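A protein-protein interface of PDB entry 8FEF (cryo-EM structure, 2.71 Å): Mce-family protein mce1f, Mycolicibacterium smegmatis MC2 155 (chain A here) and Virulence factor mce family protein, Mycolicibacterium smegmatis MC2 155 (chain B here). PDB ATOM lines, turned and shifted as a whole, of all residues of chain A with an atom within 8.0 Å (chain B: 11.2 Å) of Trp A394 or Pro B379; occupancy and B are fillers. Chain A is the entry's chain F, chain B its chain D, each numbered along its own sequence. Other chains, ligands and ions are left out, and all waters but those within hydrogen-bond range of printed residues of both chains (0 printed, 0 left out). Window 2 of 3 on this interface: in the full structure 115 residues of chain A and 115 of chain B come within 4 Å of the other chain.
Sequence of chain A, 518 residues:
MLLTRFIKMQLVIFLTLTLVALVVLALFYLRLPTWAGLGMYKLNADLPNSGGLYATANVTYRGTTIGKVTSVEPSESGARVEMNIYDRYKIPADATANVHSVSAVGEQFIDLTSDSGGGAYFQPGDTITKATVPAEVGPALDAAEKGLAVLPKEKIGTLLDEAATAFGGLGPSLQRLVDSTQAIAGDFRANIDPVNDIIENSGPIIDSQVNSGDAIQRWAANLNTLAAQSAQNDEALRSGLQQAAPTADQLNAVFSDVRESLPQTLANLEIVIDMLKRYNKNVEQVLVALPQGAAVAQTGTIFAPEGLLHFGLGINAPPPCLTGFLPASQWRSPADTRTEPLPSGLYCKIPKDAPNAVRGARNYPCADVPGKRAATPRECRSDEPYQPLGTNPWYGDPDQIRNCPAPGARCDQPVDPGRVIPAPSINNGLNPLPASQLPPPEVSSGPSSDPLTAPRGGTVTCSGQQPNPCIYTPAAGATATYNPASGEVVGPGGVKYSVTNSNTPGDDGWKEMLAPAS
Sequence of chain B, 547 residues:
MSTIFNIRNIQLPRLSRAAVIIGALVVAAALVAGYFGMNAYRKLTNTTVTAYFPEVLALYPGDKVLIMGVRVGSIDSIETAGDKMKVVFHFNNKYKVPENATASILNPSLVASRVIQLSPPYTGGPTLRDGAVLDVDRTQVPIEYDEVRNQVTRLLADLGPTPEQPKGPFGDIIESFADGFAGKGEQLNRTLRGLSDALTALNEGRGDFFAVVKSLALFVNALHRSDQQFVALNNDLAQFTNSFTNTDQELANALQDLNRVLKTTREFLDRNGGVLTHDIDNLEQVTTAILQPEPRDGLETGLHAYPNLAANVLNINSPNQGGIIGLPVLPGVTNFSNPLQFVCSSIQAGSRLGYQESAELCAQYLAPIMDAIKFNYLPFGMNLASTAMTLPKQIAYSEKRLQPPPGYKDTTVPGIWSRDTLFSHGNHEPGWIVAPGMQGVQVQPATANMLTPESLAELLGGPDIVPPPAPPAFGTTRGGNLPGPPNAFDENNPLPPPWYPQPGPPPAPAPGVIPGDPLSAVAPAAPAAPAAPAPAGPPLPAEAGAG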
ATOM      1  N   ASN A 316      -6.653 -10.724  12.399  1.00  0.00           N
ATOM      2  CA  ASN A 316      -5.241 -10.930  12.067  1.00  0.00           C
ATOM      3  C   ASN A 316      -4.585 -11.964  12.983  1.00  0.00           C
ATOM      4  O   ASN A 316      -3.482 -11.758  13.491  1.00  0.00           O
ATOM      5  CB  ASN A 316      -4.472  -9.607  12.116  1.00  0.00           C
ATOM      6  CG  ASN A 316      -4.587  -8.817  10.834  1.00  0.00           C
ATOM      7  OD1 ASN A 316      -5.442  -9.093   9.994  1.00  0.00           O
ATOM      8  ND2 ASN A 316      -3.725  -7.821  10.677  1.00  0.00           N
ATOM      9  N   PRO A 319      -1.857 -13.457   9.808  1.00  0.00           N
ATOM     10  CA  PRO A 319      -2.018 -12.485   8.733  1.00  0.00           C
ATOM     11  C   PRO A 319      -1.903 -13.159   7.379  1.00  0.00           C
ATOM     12  O   PRO A 319      -1.238 -14.201   7.244  1.00  0.00           O
ATOM     13  CB  PRO A 319      -0.861 -11.499   8.973  1.00  0.00           C
ATOM     14  CG  PRO A 319       0.164 -12.306   9.674  1.00  0.00           C
ATOM     15  CD  PRO A 319      -0.590 -13.278  10.536  1.00  0.00           C
ATOM     16  N   PRO A 320      -2.547 -12.616   6.350  1.00  0.00           N
ATOM     17  CA  PRO A 320      -2.358 -13.159   5.001  1.00  0.00           C
ATOM     18  C   PRO A 320      -0.983 -12.805   4.456  1.00  0.00           C
ATOM     19  O   PRO A 320      -0.427 -11.745   4.752  1.00  0.00           O
ATOM     20  CB  PRO A 320      -3.466 -12.481   4.191  1.00  0.00           C
ATOM     21  CG  PRO A 320      -3.673 -11.180   4.891  1.00  0.00           C
ATOM     22  CD  PRO A 320      -3.468 -11.468   6.357  1.00  0.00           C
ATOM     23  N   THR A 391      10.334 -12.206   3.082  1.00  0.00           N
ATOM     24  CA  THR A 391       9.508 -12.241   4.281  1.00  0.00           C
ATOM     25  C   THR A 391       8.354 -11.262   4.132  1.00  0.00           C
ATOM     26  O   THR A 391       8.532 -10.150   3.632  1.00  0.00           O
ATOM     27  CB  THR A 391      10.333 -11.880   5.518  1.00  0.00           C
ATOM     28  OG1 THR A 391      10.859 -10.556   5.374  1.00  0.00           O
ATOM     29  CG2 THR A 391      11.482 -12.853   5.701  1.00  0.00           C
ATOM     30  N   ASN A 392       7.165 -11.682   4.557  1.00  0.00           N
ATOM     31  CA  ASN A 392       5.979 -10.851   4.396  1.00  0.00           C
ATOM     32  C   ASN A 392       5.940  -9.764   5.465  1.00  0.00           C
ATOM     33  O   ASN A 392       5.792 -10.071   6.654  1.00  0.00           O
ATOM     34  CB  ASN A 392       4.714 -11.708   4.455  1.00  0.00           C
ATOM     35  CG  ASN A 392       3.448 -10.888   4.340  1.00  0.00           C
ATOM     36  OD1 ASN A 392       2.537 -11.016   5.156  1.00  0.00           O
ATOM     37  ND2 ASN A 392       3.385 -10.036   3.326  1.00  0.00           N
ATOM     38  N   PRO A 393       6.065  -8.495   5.088  1.00  0.00           N
ATOM     39  CA  PRO A 393       5.997  -7.414   6.070  1.00  0.00           C
ATOM     40  C   PRO A 393       4.592  -6.840   6.182  1.00  0.00           C
ATOM     41  O   PRO A 393       3.733  -7.035   5.321  1.00  0.00           O
ATOM     42  CB  PRO A 393       6.967  -6.365   5.500  1.00  0.00           C
ATOM     43  CG  PRO A 393       7.318  -6.846   4.083  1.00  0.00           C
ATOM     44  CD  PRO A 393       6.381  -7.966   3.755  1.00  0.00           C
ATOM     45  N   TRP A 394       4.369  -6.125   7.279  1.00  0.00           N
ATOM     46  CA  TRP A 394       3.104  -5.436   7.475  1.00  0.00           C
ATOM     47  C   TRP A 394       3.090  -4.048   6.851  1.00  0.00           C
ATOM     48  O   TRP A 394       2.021  -3.437   6.772  1.00  0.00           O
ATOM     49  CB  TRP A 394       2.777  -5.325   8.970  1.00  0.00           C
ATOM     50  CG  TRP A 394       3.526  -4.233   9.677  1.00  0.00           C
ATOM     51  CD1 TRP A 394       4.764  -4.323  10.238  1.00  0.00           C
ATOM     52  CD2 TRP A 394       3.084  -2.887   9.898  1.00  0.00           C
ATOM     53  NE1 TRP A 394       5.122  -3.119  10.792  1.00  0.00           N
ATOM     54  CE2 TRP A 394       4.107  -2.220  10.595  1.00  0.00           C
ATOM     55  CE3 TRP A 394       1.921  -2.180   9.570  1.00  0.00           C
ATOM     56  CZ2 TRP A 394       4.006  -0.884  10.971  1.00  0.00           C
ATOM     57  CZ3 TRP A 394       1.825  -0.854   9.941  1.00  0.00           C
ATOM     58  CH2 TRP A 394       2.860  -0.221  10.637  1.00  0.00           C
ATOM     59  N   TYR A 395       4.232  -3.555   6.371  1.00  0.00           N
ATOM     60  CA  TYR A 395       4.322  -2.181   5.891  1.00  0.00           C
ATOM     61  C   TYR A 395       4.706  -2.137   4.415  1.00  0.00           C
ATOM     62  O   TYR A 395       5.606  -1.393   4.013  1.00  0.00           O
ATOM     63  CB  TYR A 395       5.315  -1.387   6.746  1.00  0.00           C
ATOM     64  CG  TYR A 395       5.353   0.096   6.442  1.00  0.00           C
ATOM     65  CD1 TYR A 395       4.188   0.849   6.422  1.00  0.00           C
ATOM     66  CD2 TYR A 395       6.553   0.737   6.167  1.00  0.00           C
ATOM     67  CE1 TYR A 395       4.216   2.201   6.139  1.00  0.00           C
ATOM     68  CE2 TYR A 395       6.592   2.088   5.885  1.00  0.00           C
ATOM     69  CZ  TYR A 395       5.420   2.815   5.872  1.00  0.00           C
ATOM     70  OH  TYR A 395       5.454   4.162   5.591  1.00  0.00           O
ATOM     71  N   GLY A 396       4.050  -2.955   3.601  1.00  0.00           N
ATOM     72  CA  GLY A 396       4.195  -2.847   2.166  1.00  0.00           C
ATOM     73  C   GLY A 396       5.481  -3.456   1.651  1.00  0.00           C
ATOM     74  O   GLY A 396       6.320  -3.968   2.396  1.00  0.00           O
ATOM     75  N   ASP A 397       5.634  -3.372   0.333  1.00  0.00           N
ATOM     76  CA  ASP A 397       6.728  -4.005  -0.395  1.00  0.00           C
ATOM     77  C   ASP A 397       6.885  -5.490  -0.059  1.00  0.00           C
ATOM     78  O   ASP A 397       7.944  -5.915   0.413  1.00  0.00           O
ATOM     79  CB  ASP A 397       8.035  -3.260  -0.154  1.00  0.00           C
ATOM     80  CG  ASP A 397       8.027  -1.862  -0.738  1.00  0.00           C
ATOM     81  OD1 ASP A 397       7.424  -0.959  -0.120  1.00  0.00           O
ATOM     82  OD2 ASP A 397       8.624  -1.667  -1.817  1.00  0.00           O
ATOM     83  N   PRO A 398       5.848  -6.308  -0.278  1.00  0.00           N
ATOM     84  CA  PRO A 398       6.014  -7.746  -0.025  1.00  0.00           C
ATOM     85  C   PRO A 398       6.925  -8.422  -1.034  1.00  0.00           C
ATOM     86  O   PRO A 398       7.559  -9.427  -0.689  1.00  0.00           O
ATOM     87  CB  PRO A 398       4.581  -8.283  -0.105  1.00  0.00           C
ATOM     88  CG  PRO A 398       3.908  -7.369  -1.050  1.00  0.00           C
ATOM     89  CD  PRO A 398       4.515  -6.010  -0.837  1.00  0.00           C
ATOM     90  N   LEU B 330      -8.039  -8.874   6.638  1.00  0.00           N
ATOM     91  CA  LEU B 330      -8.165  -7.480   6.210  1.00  0.00           C
ATOM     92  C   LEU B 330      -6.847  -7.015   5.595  1.00  0.00           C
ATOM     93  O   LEU B 330      -6.004  -6.401   6.258  1.00  0.00           O
ATOM     94  CB  LEU B 330      -8.676  -6.612   7.371  1.00  0.00           C
ATOM     95  CG  LEU B 330      -8.082  -6.296   8.761  1.00  0.00           C
ATOM     96  CD1 LEU B 330      -7.003  -5.218   8.812  1.00  0.00           C
ATOM     97  CD2 LEU B 330      -9.204  -5.961   9.736  1.00  0.00           C
ATOM     98  N   PRO B 331      -6.618  -7.332   4.317  1.00  0.00           N
ATOM     99  CA  PRO B 331      -5.408  -6.847   3.641  1.00  0.00           C
ATOM    100  C   PRO B 331      -5.505  -5.373   3.282  1.00  0.00           C
ATOM    101  O   PRO B 331      -6.472  -4.699   3.646  1.00  0.00           O
ATOM    102  CB  PRO B 331      -5.330  -7.722   2.383  1.00  0.00           C
ATOM    103  CG  PRO B 331      -6.290  -8.849   2.614  1.00  0.00           C
ATOM    104  CD  PRO B 331      -7.359  -8.292   3.486  1.00  0.00           C
ATOM    105  N   GLY B 332      -4.504  -4.864   2.572  1.00  0.00           N
ATOM    106  CA  GLY B 332      -4.511  -3.480   2.133  1.00  0.00           C
ATOM    107  C   GLY B 332      -4.264  -2.484   3.247  1.00  0.00           C
ATOM    108  O   GLY B 332      -4.229  -1.276   3.014  1.00  0.00           O
ATOM    109  N   PHE B 375       0.247   0.144   4.062  1.00  0.00           N
ATOM    110  CA  PHE B 375       0.622  -1.017   4.860  1.00  0.00           C
ATOM    111  C   PHE B 375      -0.156  -2.250   4.419  1.00  0.00           C
ATOM    112  O   PHE B 375      -1.289  -2.141   3.957  1.00  0.00           O
ATOM    113  CB  PHE B 375       0.394  -0.739   6.350  1.00  0.00           C
ATOM    114  CG  PHE B 375      -1.035  -0.422   6.705  1.00  0.00           C
ATOM    115  CD1 PHE B 375      -1.499   0.882   6.663  1.00  0.00           C
ATOM    116  CD2 PHE B 375      -1.904  -1.422   7.104  1.00  0.00           C
ATOM    117  CE1 PHE B 375      -2.806   1.178   6.994  1.00  0.00           C
ATOM    118  CE2 PHE B 375      -3.212  -1.131   7.436  1.00  0.00           C
ATOM    119  CZ  PHE B 375      -3.662   0.170   7.382  1.00  0.00           C
ATOM    120  N   ASN B 376       0.461  -3.424   4.555  1.00  0.00           N
ATOM    121  CA  ASN B 376      -0.203  -4.657   4.143  1.00  0.00           C
ATOM    122  C   ASN B 376      -1.354  -5.006   5.077  1.00  0.00           C
ATOM    123  O   ASN B 376      -2.458  -5.327   4.623  1.00  0.00           O
ATOM    124  CB  ASN B 376       0.805  -5.804   4.078  1.00  0.00           C
ATOM    125  CG  ASN B 376       1.819  -5.625   2.972  1.00  0.00           C
ATOM    126  OD1 ASN B 376       1.626  -4.820   2.063  1.00  0.00           O
ATOM    127  ND2 ASN B 376       2.907  -6.381   3.039  1.00  0.00           N
ATOM    128  N   TYR B 377      -1.119  -4.945   6.385  1.00  0.00           N
ATOM    129  CA  TYR B 377      -2.149  -5.265   7.365  1.00  0.00           C
ATOM    130  C   TYR B 377      -1.778  -4.621   8.695  1.00  0.00           C
ATOM    131  O   TYR B 377      -0.794  -3.884   8.800  1.00  0.00           O
ATOM    132  CB  TYR B 377      -2.333  -6.780   7.497  1.00  0.00           C
ATOM    133  CG  TYR B 377      -1.045  -7.555   7.639  1.00  0.00           C
ATOM    134  CD1 TYR B 377      -0.417  -7.678   8.869  1.00  0.00           C
ATOM    135  CD2 TYR B 377      -0.463  -8.174   6.544  1.00  0.00           C
ATOM    136  CE1 TYR B 377       0.759  -8.385   9.003  1.00  0.00           C
ATOM    137  CE2 TYR B 377       0.712  -8.886   6.670  1.00  0.00           C
ATOM    138  CZ  TYR B 377       1.317  -8.988   7.903  1.00  0.00           C
ATOM    139  OH  TYR B 377       2.488  -9.696   8.037  1.00  0.00           O
ATOM    140  N   LEU B 378      -2.585  -4.904   9.713  1.00  0.00           N
ATOM    141  CA  LEU B 378      -2.398  -4.282  11.014  1.00  0.00           C
ATOM    142  C   LEU B 378      -1.201  -4.895  11.738  1.00  0.00           C
ATOM    143  O   LEU B 378      -0.965  -6.102  11.634  1.00  0.00           O
ATOM    144  CB  LEU B 378      -3.656  -4.435  11.866  1.00  0.00           C
ATOM    145  CG  LEU B 378      -4.867  -3.619  11.420  1.00  0.00           C
ATOM    146  CD1 LEU B 378      -6.049  -3.882  12.337  1.00  0.00           C
ATOM    147  CD2 LEU B 378      -4.526  -2.141  11.390  1.00  0.00           C
ATOM    148  N   PRO B 379      -0.430  -4.090  12.474  1.00  0.00           N
ATOM    149  CA  PRO B 379       0.739  -4.632  13.188  1.00  0.00           C
ATOM    150  C   PRO B 379       0.387  -5.634  14.270  1.00  0.00           C
ATOM    151  O   PRO B 379       1.242  -6.446  14.638  1.00  0.00           O
ATOM    152  CB  PRO B 379       1.397  -3.382  13.789  1.00  0.00           C
ATOM    153  CG  PRO B 379       0.842  -2.236  13.023  1.00  0.00           C
ATOM    154  CD  PRO B 379      -0.543  -2.632  12.632  1.00  0.00           C
ATOM    155  N   PHE B 380      -0.835  -5.606  14.790  1.00  0.00           N
ATOM    156  CA  PHE B 380      -1.228  -6.431  15.919  1.00  0.00           C
ATOM    157  C   PHE B 380      -2.361  -7.368  15.526  1.00  0.00           C
ATOM    158  O   PHE B 380      -3.124  -7.095  14.596  1.00  0.00           O
ATOM    159  CB  PHE B 380      -1.658  -5.567  17.109  1.00  0.00           C
ATOM    160  CG  PHE B 380      -2.490  -4.376  16.726  1.00  0.00           C
ATOM    161  CD1 PHE B 380      -3.833  -4.519  16.416  1.00  0.00           C
ATOM    162  CD2 PHE B 380      -1.931  -3.110  16.685  1.00  0.00           C
ATOM    163  CE1 PHE B 380      -4.597  -3.426  16.066  1.00  0.00           C
ATOM    164  CE2 PHE B 380      -2.691  -2.013  16.337  1.00  0.00           C
ATOM    165  CZ  PHE B 380      -4.027  -2.172  16.027  1.00  0.00           C
ATOM    166  N   GLY B 381      -2.459  -8.478  16.249  1.00  0.00           N
ATOM    167  CA  GLY B 381      -3.513  -9.446  16.017  1.00  0.00           C
ATOM    168  C   GLY B 381      -3.928 -10.087  17.322  1.00  0.00           C
ATOM    169  O   GLY B 381      -3.201 -10.042  18.318  1.00  0.00           O
ATOM    170  N   MET B 382      -5.115 -10.690  17.308  1.00  0.00           N
ATOM    171  CA  MET B 382      -5.676 -11.281  18.511  1.00  0.00           C
ATOM    172  C   MET B 382      -6.431 -12.554  18.166  1.00  0.00           C
ATOM    173  O   MET B 382      -7.088 -12.634  17.124  1.00  0.00           O
ATOM    174  CB  MET B 382      -6.607 -10.298  19.229  1.00  0.00           C
ATOM    175  CG  MET B 382      -6.763 -10.563  20.716  1.00  0.00           C
ATOM    176  SD  MET B 382      -7.442  -9.145  21.598  1.00  0.00           S
ATOM    177  CE  MET B 382      -6.924  -9.510  23.273  1.00  0.00           C
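Among the printed residues, merely in contact across the chains: Asn A316 with Tyr B377 (3.6 Å), Asn A316 with Phe B380 (3.8 Å), Asn A316 with Gly B381 (3.4 Å), Pro A319 with Tyr B377 (3.5 Å), Pro A320 with Tyr B377 (3.6 Å), Asn A392 with Asn B376 (3.7 Å), Pro A393 with Tyr B377 (3.8 Å), Trp A394 with Phe B375 (3.2 Å) and Trp A394 with Pro B379 (3.5 Å).
Printed residues of chain A that touch a printed residue of chain B: Asn A316, Pro A319, Pro A320, Asn A392, Pro A393, Trp A394 and Gly A396. Of the 11 printed residues of chain B, 7 touch a printed residue of chain A. Along chain B the printed residues that touch a printed residue of chain A span positions 375 to 381. Among the printed residues, 15 pairs touch across the chains. Among the printed residues, no Asp or Glu carboxylate lies within 4 Å of a Lys or Arg side-chain nitrogen of the other chain.
N of Gly B332 is in hydrogen-bond range of O of Asn B376 (2.9 Å). The backbone carbonyl oxygen (O) of Pro A320 lies close to the side-chain amide oxygen (OD1) of Asn A392 (3.1 Å).
The backbone carbonyl oxygen of Tyr B377 lies close to the backbone carbonyl oxygen of Trp A394 (3.5 Å). The side-chain amide nitrogen of Asn A316 sits close to the backbone NH of Leu B378 (3.3 Å). OH of Tyr B377 sits at hydrogen-bond distance from OD1 of Asn A392 (3.2 Å). The side-chain amide oxygen (OD1) of Asn B376 sits close to the backbone NH (N) of Gly A396, 3.4 Å away. ND2 of Asn B376 sits at hydrogen-bond distance from O of Pro A393, at 2.5 Å. N of Asn B376 sits at hydrogen-bond distance from O of Trp A394.
Of the printed residues of chain B, Asn A316 touches Tyr B377, Leu B378, Phe B380 and Gly B381. Of chain B, only Asn B376 and Tyr B377 come within 4 Å of Asn A392. Printed residues of chain B within 4 Å of Trp A394: Phe B375, Asn B376, Tyr B377 and Pro B379. Asp A397 touches none of the printed residues of chain B. Gly B332 touches none of the printed residues of chain A. Of the printed residues of chain A, Tyr B377 touches Asn A316, Pro A319, Pro A320, Asn A392, Pro A393 and Trp A394. Pro B379 touches just one residue of chain A: Trp A394. Printed residues of chain A within 4 Å of Phe B380: Asn A316. The nearest residue of chain B that does not touch Trp A394 is Leu B378 (4.7 Å). The nearest residue of chain A that does not touch Pro B379 is Asn A316 (5.3 Å).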
